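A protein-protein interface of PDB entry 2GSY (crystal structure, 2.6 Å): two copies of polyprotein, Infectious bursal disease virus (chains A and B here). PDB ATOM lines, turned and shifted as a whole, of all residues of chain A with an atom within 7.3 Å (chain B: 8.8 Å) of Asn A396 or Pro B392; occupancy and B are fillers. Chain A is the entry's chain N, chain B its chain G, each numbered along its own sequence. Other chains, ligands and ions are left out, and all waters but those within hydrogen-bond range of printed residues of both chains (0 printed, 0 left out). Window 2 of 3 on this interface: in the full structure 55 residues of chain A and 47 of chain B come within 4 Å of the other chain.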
ATOM      1  N   PRO A  29      21.288 -15.258  12.167  1.00  0.00           N
ATOM      2  CA  PRO A  29      20.166 -16.187  12.123  1.00  0.00           C
ATOM      3  C   PRO A  29      18.826 -15.486  11.902  1.00  0.00           C
ATOM      4  O   PRO A  29      17.885 -15.702  12.664  1.00  0.00           O
ATOM      5  CB  PRO A  29      20.213 -16.830  13.508  1.00  0.00           C
ATOM      6  CG  PRO A  29      20.732 -15.740  14.396  1.00  0.00           C
ATOM      7  CD  PRO A  29      21.591 -14.832  13.546  1.00  0.00           C
ATOM      8  N   ASP A 391      20.701 -23.120  13.067  1.00  0.00           N
ATOM      9  CA  ASP A 391      20.387 -23.500  14.433  1.00  0.00           C
ATOM     10  C   ASP A 391      19.246 -22.688  15.013  1.00  0.00           C
ATOM     11  O   ASP A 391      19.327 -21.466  15.138  1.00  0.00           O
ATOM     12  CB  ASP A 391      21.608 -23.588  15.367  1.00  0.00           C
ATOM     13  CG  ASP A 391      22.303 -22.272  15.559  1.00  0.00           C
ATOM     14  OD1 ASP A 391      22.254 -21.443  14.629  1.00  0.00           O
ATOM     15  OD2 ASP A 391      22.909 -22.078  16.638  1.00  0.00           O
ATOM     16  N   PRO A 392      18.167 -23.391  15.369  1.00  0.00           N
ATOM     17  CA  PRO A 392      16.959 -22.771  15.876  1.00  0.00           C
ATOM     18  C   PRO A 392      17.266 -22.256  17.272  1.00  0.00           C
ATOM     19  O   PRO A 392      18.130 -22.810  17.960  1.00  0.00           O
ATOM     20  CB  PRO A 392      15.978 -23.944  15.940  1.00  0.00           C
ATOM     21  CG  PRO A 392      16.848 -25.148  16.146  1.00  0.00           C
ATOM     22  CD  PRO A 392      18.088 -24.866  15.366  1.00  0.00           C
ATOM     23  N   GLY A 393      16.595 -21.198  17.692  1.00  0.00           N
ATOM     24  CA  GLY A 393      16.871 -20.659  19.010  1.00  0.00           C
ATOM     25  C   GLY A 393      18.077 -19.742  19.058  1.00  0.00           C
ATOM     26  O   GLY A 393      18.299 -19.091  20.070  1.00  0.00           O
ATOM     27  N   ALA A 394      18.854 -19.681  17.978  1.00  0.00           N
ATOM     28  CA  ALA A 394      19.952 -18.722  17.892  1.00  0.00           C
ATOM     29  C   ALA A 394      19.427 -17.293  17.947  1.00  0.00           C
ATOM     30  O   ALA A 394      19.930 -16.473  18.714  1.00  0.00           O
ATOM     31  CB  ALA A 394      20.775 -18.941  16.633  1.00  0.00           C
ATOM     32  N   MET A 395      18.407 -17.002  17.144  1.00  0.00           N
ATOM     33  CA  MET A 395      17.830 -15.662  17.101  1.00  0.00           C
ATOM     34  C   MET A 395      17.096 -15.315  18.396  1.00  0.00           C
ATOM     35  O   MET A 395      17.207 -14.189  18.886  1.00  0.00           O
ATOM     36  CB  MET A 395      16.919 -15.484  15.880  1.00  0.00           C
ATOM     37  CG  MET A 395      16.273 -14.113  15.777  1.00  0.00           C
ATOM     38  SD  MET A 395      17.467 -12.768  15.816  1.00  0.00           S
ATOM     39  CE  MET A 395      17.859 -12.591  14.081  1.00  0.00           C
ATOM     40  N   ASN A 396      16.365 -16.278  18.955  1.00  0.00           N
ATOM     41  CA  ASN A 396      15.663 -16.060  20.217  1.00  0.00           C
ATOM     42  C   ASN A 396      16.647 -15.779  21.324  1.00  0.00           C
ATOM     43  O   ASN A 396      16.403 -14.937  22.182  1.00  0.00           O
ATOM     44  CB  ASN A 396      14.820 -17.272  20.615  1.00  0.00           C
ATOM     45  CG  ASN A 396      13.698 -17.556  19.644  1.00  0.00           C
ATOM     46  OD1 ASN A 396      12.552 -17.731  20.049  1.00  0.00           O
ATOM     47  ND2 ASN A 396      14.023 -17.628  18.354  1.00  0.00           N
ATOM     48  N   TYR A 397      17.765 -16.495  21.299  1.00  0.00           N
ATOM     49  CA  TYR A 397      18.798 -16.316  22.295  1.00  0.00           C
ATOM     50  C   TYR A 397      19.426 -14.933  22.169  1.00  0.00           C
ATOM     51  O   TYR A 397      19.671 -14.265  23.169  1.00  0.00           O
ATOM     52  CB  TYR A 397      19.845 -17.421  22.185  1.00  0.00           C
ATOM     53  CG  TYR A 397      20.755 -17.486  23.380  1.00  0.00           C
ATOM     54  CD1 TYR A 397      20.343 -18.095  24.566  1.00  0.00           C
ATOM     55  CD2 TYR A 397      22.027 -16.923  23.332  1.00  0.00           C
ATOM     56  CE1 TYR A 397      21.186 -18.142  25.674  1.00  0.00           C
ATOM     57  CE2 TYR A 397      22.873 -16.962  24.427  1.00  0.00           C
ATOM     58  CZ  TYR A 397      22.452 -17.571  25.593  1.00  0.00           C
ATOM     59  OH  TYR A 397      23.309 -17.602  26.666  1.00  0.00           O
ATOM     60  N   THR A 398      19.656 -14.503  20.934  1.00  0.00           N
ATOM     61  CA  THR A 398      20.158 -13.161  20.656  1.00  0.00           C
ATOM     62  C   THR A 398      19.190 -12.109  21.179  1.00  0.00           C
ATOM     63  O   THR A 398      19.598 -11.133  21.817  1.00  0.00           O
ATOM     64  CB  THR A 398      20.357 -12.962  19.150  1.00  0.00           C
ATOM     65  OG1 THR A 398      21.155 -14.033  18.640  1.00  0.00           O
ATOM     66  CG2 THR A 398      21.043 -11.638  18.857  1.00  0.00           C
ATOM     67  N   LYS A 399      17.904 -12.324  20.910  1.00  0.00           N
ATOM     68  CA  LYS A 399      16.860 -11.402  21.328  1.00  0.00           C
ATOM     69  C   LYS A 399      16.791 -11.315  22.842  1.00  0.00           C
ATOM     70  O   LYS A 399      16.609 -10.231  23.388  1.00  0.00           O
ATOM     71  CB  LYS A 399      15.509 -11.822  20.754  1.00  0.00           C
ATOM     72  CG  LYS A 399      15.315 -11.421  19.312  1.00  0.00           C
ATOM     73  CD  LYS A 399      14.086 -12.077  18.733  1.00  0.00           C
ATOM     74  CE  LYS A 399      13.945 -11.745  17.265  1.00  0.00           C
ATOM     75  NZ  LYS A 399      12.742 -12.392  16.691  1.00  0.00           N
ATOM     76  N   LEU A 400      16.948 -12.458  23.505  1.00  0.00           N
ATOM     77  CA  LEU A 400      16.960 -12.524  24.959  1.00  0.00           C
ATOM     78  C   LEU A 400      18.133 -11.751  25.531  1.00  0.00           C
ATOM     79  O   LEU A 400      17.963 -10.929  26.428  1.00  0.00           O
ATOM     80  CB  LEU A 400      17.025 -13.978  25.433  1.00  0.00           C
ATOM     81  CG  LEU A 400      17.207 -14.217  26.936  1.00  0.00           C
ATOM     82  CD1 LEU A 400      16.034 -13.679  27.737  1.00  0.00           C
ATOM     83  CD2 LEU A 400      17.396 -15.693  27.218  1.00  0.00           C
ATOM     84  N   ILE A 401      19.321 -12.033  25.004  1.00  0.00           N
ATOM     85  CA  ILE A 401      20.552 -11.384  25.433  1.00  0.00           C
ATOM     86  C   ILE A 401      20.421  -9.874  25.311  1.00  0.00           C
ATOM     87  O   ILE A 401      20.686  -9.150  26.265  1.00  0.00           O
ATOM     88  CB  ILE A 401      21.771 -11.896  24.613  1.00  0.00           C
ATOM     89  CG1 ILE A 401      22.108 -13.347  24.975  1.00  0.00           C
ATOM     90  CG2 ILE A 401      22.992 -11.008  24.799  1.00  0.00           C
ATOM     91  CD1 ILE A 401      22.244 -13.615  26.457  1.00  0.00           C
ATOM     92  N   LEU A 402      19.992  -9.411  24.142  1.00  0.00           N
ATOM     93  CA  LEU A 402      19.853  -7.982  23.889  1.00  0.00           C
ATOM     94  C   LEU A 402      18.758  -7.367  24.742  1.00  0.00           C
ATOM     95  O   LEU A 402      18.879  -6.236  25.204  1.00  0.00           O
ATOM     96  CB  LEU A 402      19.580  -7.723  22.412  1.00  0.00           C
ATOM     97  CG  LEU A 402      20.729  -8.060  21.460  1.00  0.00           C
ATOM     98  CD1 LEU A 402      20.275  -7.842  20.041  1.00  0.00           C
ATOM     99  CD2 LEU A 402      21.975  -7.238  21.762  1.00  0.00           C
ATOM    100  N   SER A 403      17.696  -8.124  24.960  1.00  0.00           N
ATOM    101  CA  SER A 403      16.613  -7.693  25.815  1.00  0.00           C
ATOM    102  C   SER A 403      17.105  -7.421  27.238  1.00  0.00           C
ATOM    103  O   SER A 403      16.563  -6.566  27.934  1.00  0.00           O
ATOM    104  CB  SER A 403      15.518  -8.751  25.797  1.00  0.00           C
ATOM    105  OG  SER A 403      14.806  -8.799  27.009  1.00  0.00           O
ATOM    106  N   ILE B  11      -1.169 -11.989  29.320  1.00  0.00           N
ATOM    107  CA  ILE B  11      -1.474 -11.983  27.871  1.00  0.00           C
ATOM    108  C   ILE B  11      -0.160 -11.823  27.113  1.00  0.00           C
ATOM    109  O   ILE B  11       0.873 -12.349  27.535  1.00  0.00           O
ATOM    110  CB  ILE B  11      -2.572 -10.962  27.374  1.00  0.00           C
ATOM    111  CG1 ILE B  11      -2.612  -9.677  28.213  1.00  0.00           C
ATOM    112  CG2 ILE B  11      -3.952 -11.639  27.290  1.00  0.00           C
ATOM    113  CD1 ILE B  11      -3.666  -8.663  27.725  1.00  0.00           C
ATOM    114  N   VAL B  12      -0.191 -11.120  25.993  1.00  0.00           N
ATOM    115  CA  VAL B  12       1.023 -10.867  25.244  1.00  0.00           C
ATOM    116  C   VAL B  12       1.023  -9.376  24.942  1.00  0.00           C
ATOM    117  O   VAL B  12       0.232  -8.918  24.117  1.00  0.00           O
ATOM    118  CB  VAL B  12       1.093 -11.730  23.952  1.00  0.00           C
ATOM    119  CG1 VAL B  12       2.300 -11.355  23.109  1.00  0.00           C
ATOM    120  CG2 VAL B  12       1.124 -13.226  24.293  1.00  0.00           C
ATOM    121  N   PRO B  29       7.354  -7.688  17.857  1.00  0.00           N
ATOM    122  CA  PRO B  29       8.246  -8.823  18.071  1.00  0.00           C
ATOM    123  C   PRO B  29       8.790  -9.404  16.766  1.00  0.00           C
ATOM    124  O   PRO B  29       8.684 -10.609  16.535  1.00  0.00           O
ATOM    125  CB  PRO B  29       7.340  -9.835  18.770  1.00  0.00           C
ATOM    126  CG  PRO B  29       5.982  -9.564  18.191  1.00  0.00           C
ATOM    127  CD  PRO B  29       5.942  -8.110  17.776  1.00  0.00           C
ATOM    128  N   ASP B  31      12.211  -9.010  13.707  1.00  0.00           N
ATOM    129  CA  ASP B  31      13.666  -9.149  13.729  1.00  0.00           C
ATOM    130  C   ASP B  31      14.389  -7.808  13.639  1.00  0.00           C
ATOM    131  O   ASP B  31      15.619  -7.752  13.607  1.00  0.00           O
ATOM    132  CB  ASP B  31      14.114 -10.077  12.603  1.00  0.00           C
ATOM    133  CG  ASP B  31      13.425 -11.423  12.659  1.00  0.00           C
ATOM    134  OD1 ASP B  31      13.652 -12.167  13.636  1.00  0.00           O
ATOM    135  OD2 ASP B  31      12.654 -11.736  11.726  1.00  0.00           O
ATOM    136  N   LEU B  33      15.798  -5.450  15.315  1.00  0.00           N
ATOM    137  CA  LEU B  33      16.336  -5.157  16.636  1.00  0.00           C
ATOM    138  C   LEU B  33      17.118  -3.850  16.719  1.00  0.00           C
ATOM    139  O   LEU B  33      18.334  -3.830  16.533  1.00  0.00           O
ATOM    140  CB  LEU B  33      17.224  -6.303  17.108  1.00  0.00           C
ATOM    141  CG  LEU B  33      16.584  -7.670  17.320  1.00  0.00           C
ATOM    142  CD1 LEU B  33      17.634  -8.601  17.870  1.00  0.00           C
ATOM    143  CD2 LEU B  33      15.378  -7.603  18.261  1.00  0.00           C
ATOM    144  N   ARG B 389      11.560  -5.762  24.729  1.00  0.00           N
ATOM    145  CA  ARG B 389      11.337  -6.892  25.630  1.00  0.00           C
ATOM    146  C   ARG B 389      11.259  -8.165  24.816  1.00  0.00           C
ATOM    147  O   ARG B 389      10.596  -8.216  23.780  1.00  0.00           O
ATOM    148  CB  ARG B 389      10.041  -6.736  26.440  1.00  0.00           C
ATOM    149  CG  ARG B 389      10.022  -5.635  27.518  1.00  0.00           C
ATOM    150  CD  ARG B 389      11.303  -5.588  28.374  1.00  0.00           C
ATOM    151  NE  ARG B 389      12.354  -4.785  27.733  1.00  0.00           N
ATOM    152  CZ  ARG B 389      13.627  -4.715  28.130  1.00  0.00           C
ATOM    153  NH1 ARG B 389      14.052  -5.400  29.188  1.00  0.00           N
ATOM    154  NH2 ARG B 389      14.480  -3.949  27.457  1.00  0.00           N
ATOM    155  N   PHE B 390      11.953  -9.189  25.280  1.00  0.00           N
ATOM    156  CA  PHE B 390      11.894 -10.464  24.619  1.00  0.00           C
ATOM    157  C   PHE B 390      10.744 -11.264  25.182  1.00  0.00           C
ATOM    158  O   PHE B 390      10.735 -11.588  26.370  1.00  0.00           O
ATOM    159  CB  PHE B 390      13.198 -11.232  24.834  1.00  0.00           C
ATOM    160  CG  PHE B 390      13.168 -12.643  24.317  1.00  0.00           C
ATOM    161  CD1 PHE B 390      12.935 -12.902  22.966  1.00  0.00           C
ATOM    162  CD2 PHE B 390      13.377 -13.713  25.179  1.00  0.00           C
ATOM    163  CE1 PHE B 390      12.910 -14.208  22.484  1.00  0.00           C
ATOM    164  CE2 PHE B 390      13.360 -15.021  24.710  1.00  0.00           C
ATOM    165  CZ  PHE B 390      13.127 -15.271  23.360  1.00  0.00           C
ATOM    166  N   ASP B 391       9.760 -11.568  24.347  1.00  0.00           N
ATOM    167  CA  ASP B 391       8.934 -12.731  24.633  1.00  0.00           C
ATOM    168  C   ASP B 391       8.697 -13.590  23.409  1.00  0.00           C
ATOM    169  O   ASP B 391       8.116 -13.145  22.417  1.00  0.00           O
ATOM    170  CB  ASP B 391       7.648 -12.424  25.422  1.00  0.00           C
ATOM    171  CG  ASP B 391       6.694 -11.540  24.674  1.00  0.00           C
ATOM    172  OD1 ASP B 391       7.166 -10.727  23.854  1.00  0.00           O
ATOM    173  OD2 ASP B 391       5.471 -11.653  24.919  1.00  0.00           O
ATOM    174  N   PRO B 392       9.162 -14.841  23.490  1.00  0.00           N
ATOM    175  CA  PRO B 392       9.084 -15.780  22.389  1.00  0.00           C
ATOM    176  C   PRO B 392       7.626 -16.176  22.233  1.00  0.00           C
ATOM    177  O   PRO B 392       6.870 -16.156  23.209  1.00  0.00           O
ATOM    178  CB  PRO B 392       9.909 -16.963  22.890  1.00  0.00           C
ATOM    179  CG  PRO B 392       9.781 -16.903  24.385  1.00  0.00           C
ATOM    180  CD  PRO B 392       9.738 -15.444  24.706  1.00  0.00           C
ATOM    181  N   GLY B 393       7.211 -16.513  21.025  1.00  0.00           N
ATOM    182  CA  GLY B 393       5.820 -16.874  20.830  1.00  0.00           C
ATOM    183  C   GLY B 393       4.892 -15.685  20.670  1.00  0.00           C
ATOM    184  O   GLY B 393       3.731 -15.866  20.319  1.00  0.00           O
ATOM    185  N   ALA B 394       5.389 -14.474  20.916  1.00  0.00           N
ATOM    186  CA  ALA B 394       4.603 -13.272  20.651  1.00  0.00           C
ATOM    187  C   ALA B 394       4.280 -13.149  19.164  1.00  0.00           C
ATOM    188  O   ALA B 394       3.128 -12.925  18.792  1.00  0.00           O
ATOM    189  CB  ALA B 394       5.322 -12.023  21.150  1.00  0.00           C
ATOM    190  N   MET B 395       5.297 -13.308  18.319  1.00  0.00           N
ATOM    191  CA  MET B 395       5.106 -13.203  16.877  1.00  0.00           C
ATOM    192  C   MET B 395       4.271 -14.362  16.322  1.00  0.00           C
ATOM    193  O   MET B 395       3.415 -14.150  15.466  1.00  0.00           O
ATOM    194  CB  MET B 395       6.446 -13.089  16.149  1.00  0.00           C
ATOM    195  CG  MET B 395       6.325 -12.989  14.637  1.00  0.00           C
ATOM    196  SD  MET B 395       5.250 -11.645  14.104  1.00  0.00           S
ATOM    197  CE  MET B 395       6.418 -10.289  13.988  1.00  0.00           C
ATOM    198  N   ASN B 396       4.508 -15.574  16.821  1.00  0.00           N
ATOM    199  CA  ASN B 396       3.728 -16.734  16.393  1.00  0.00           C
ATOM    200  C   ASN B 396       2.274 -16.559  16.760  1.00  0.00           C
ATOM    201  O   ASN B 396       1.386 -16.923  15.995  1.00  0.00           O
ATOM    202  CB  ASN B 396       4.237 -18.026  17.031  1.00  0.00           C
ATOM    203  CG  ASN B 396       5.644 -18.379  16.607  1.00  0.00           C
ATOM    204  OD1 ASN B 396       5.908 -19.506  16.207  1.00  0.00           O
ATOM    205  ND2 ASN B 396       6.561 -17.423  16.714  1.00  0.00           N
ATOM    206  N   TYR B 397       2.040 -16.003  17.941  1.00  0.00           N
ATOM    207  CA  TYR B 397       0.693 -15.767  18.407  1.00  0.00           C
ATOM    208  C   TYR B 397       0.003 -14.722  17.534  1.00  0.00           C
ATOM    209  O   TYR B 397      -1.161 -14.874  17.180  1.00  0.00           O
ATOM    210  CB  TYR B 397       0.700 -15.358  19.879  1.00  0.00           C
ATOM    211  CG  TYR B 397      -0.662 -15.415  20.509  1.00  0.00           C
ATOM    212  CD1 TYR B 397      -1.211 -16.628  20.927  1.00  0.00           C
ATOM    213  CD2 TYR B 397      -1.415 -14.257  20.674  1.00  0.00           C
ATOM    214  CE1 TYR B 397      -2.479 -16.679  21.502  1.00  0.00           C
ATOM    215  CE2 TYR B 397      -2.679 -14.293  21.244  1.00  0.00           C
ATOM    216  CZ  TYR B 397      -3.206 -15.502  21.655  1.00  0.00           C
ATOM    217  OH  TYR B 397      -4.459 -15.514  22.218  1.00  0.00           O
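Asn A396 touches Pro B392, but with the chains exchanged Pro A392 does not touch Asn B396 (11.0 Å).
8 positions are printed for both chains.
The backbone carbonyl oxygen of Ser A403 sits at hydrogen-bond distance from the guanidinium group of Arg B389 (3.0 Å).
The side-chain amino group of Lys A399 is in salt-bridge range of the side-chain carboxylate of Asp B31.
The backbone NH of Phe B390 sits at hydrogen-bond distance from the side-chain hydroxyl of Ser A403, at 3.4 Å.
Among the printed residues, pairs that only touch across the chains: Met A395 with Asp B31 (3.9 Å), Asn A396 with Phe B390 (3.5 Å), Asn A396 with Pro B392 (3.96 Å), Lys A399 with Leu B33 (3.9 Å), Lys A399 with Phe B390 (3.6 Å), Leu A400 with Phe B390 (3.7 Å) and Leu A402 with Leu B33 (3.5 Å).
Among the printed residues, 10 pairs touch across the chains.
Among the printed residues, Asp or Glu carboxylates within 4 Å of a Lys or Arg side-chain nitrogen of the other chain: Lys A399 with Asp B31 (3.2 Å).
Asn A396 touches just these residues of chain B: Phe B390 and Pro B392.
Pro B392 touches just one residue of chain A: Asn A396.
No residue of chain B comes within 4 Å of Gly A393.
Printed residues of chain B within 4 Å of Lys A399: Asp B31, Leu B33 and Phe B390.
Printed residues of chain A within 4 Å of Phe B390: Asn A396 (3.5 Å), Lys A399 (3.6 Å), Leu A400 (3.7 Å) and Ser A403 (3.4 Å).
Printed residues of chain A within 4 Å of Leu B33: Lys A399 (3.9 Å) and Leu A402 (3.5 Å).
Printed residues of chain A within 4 Å of Arg B389: Ser A403 (3.0 Å).
The nearest residue of chain B that does not touch Asn A396 is Gly B393 (5.6 Å).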
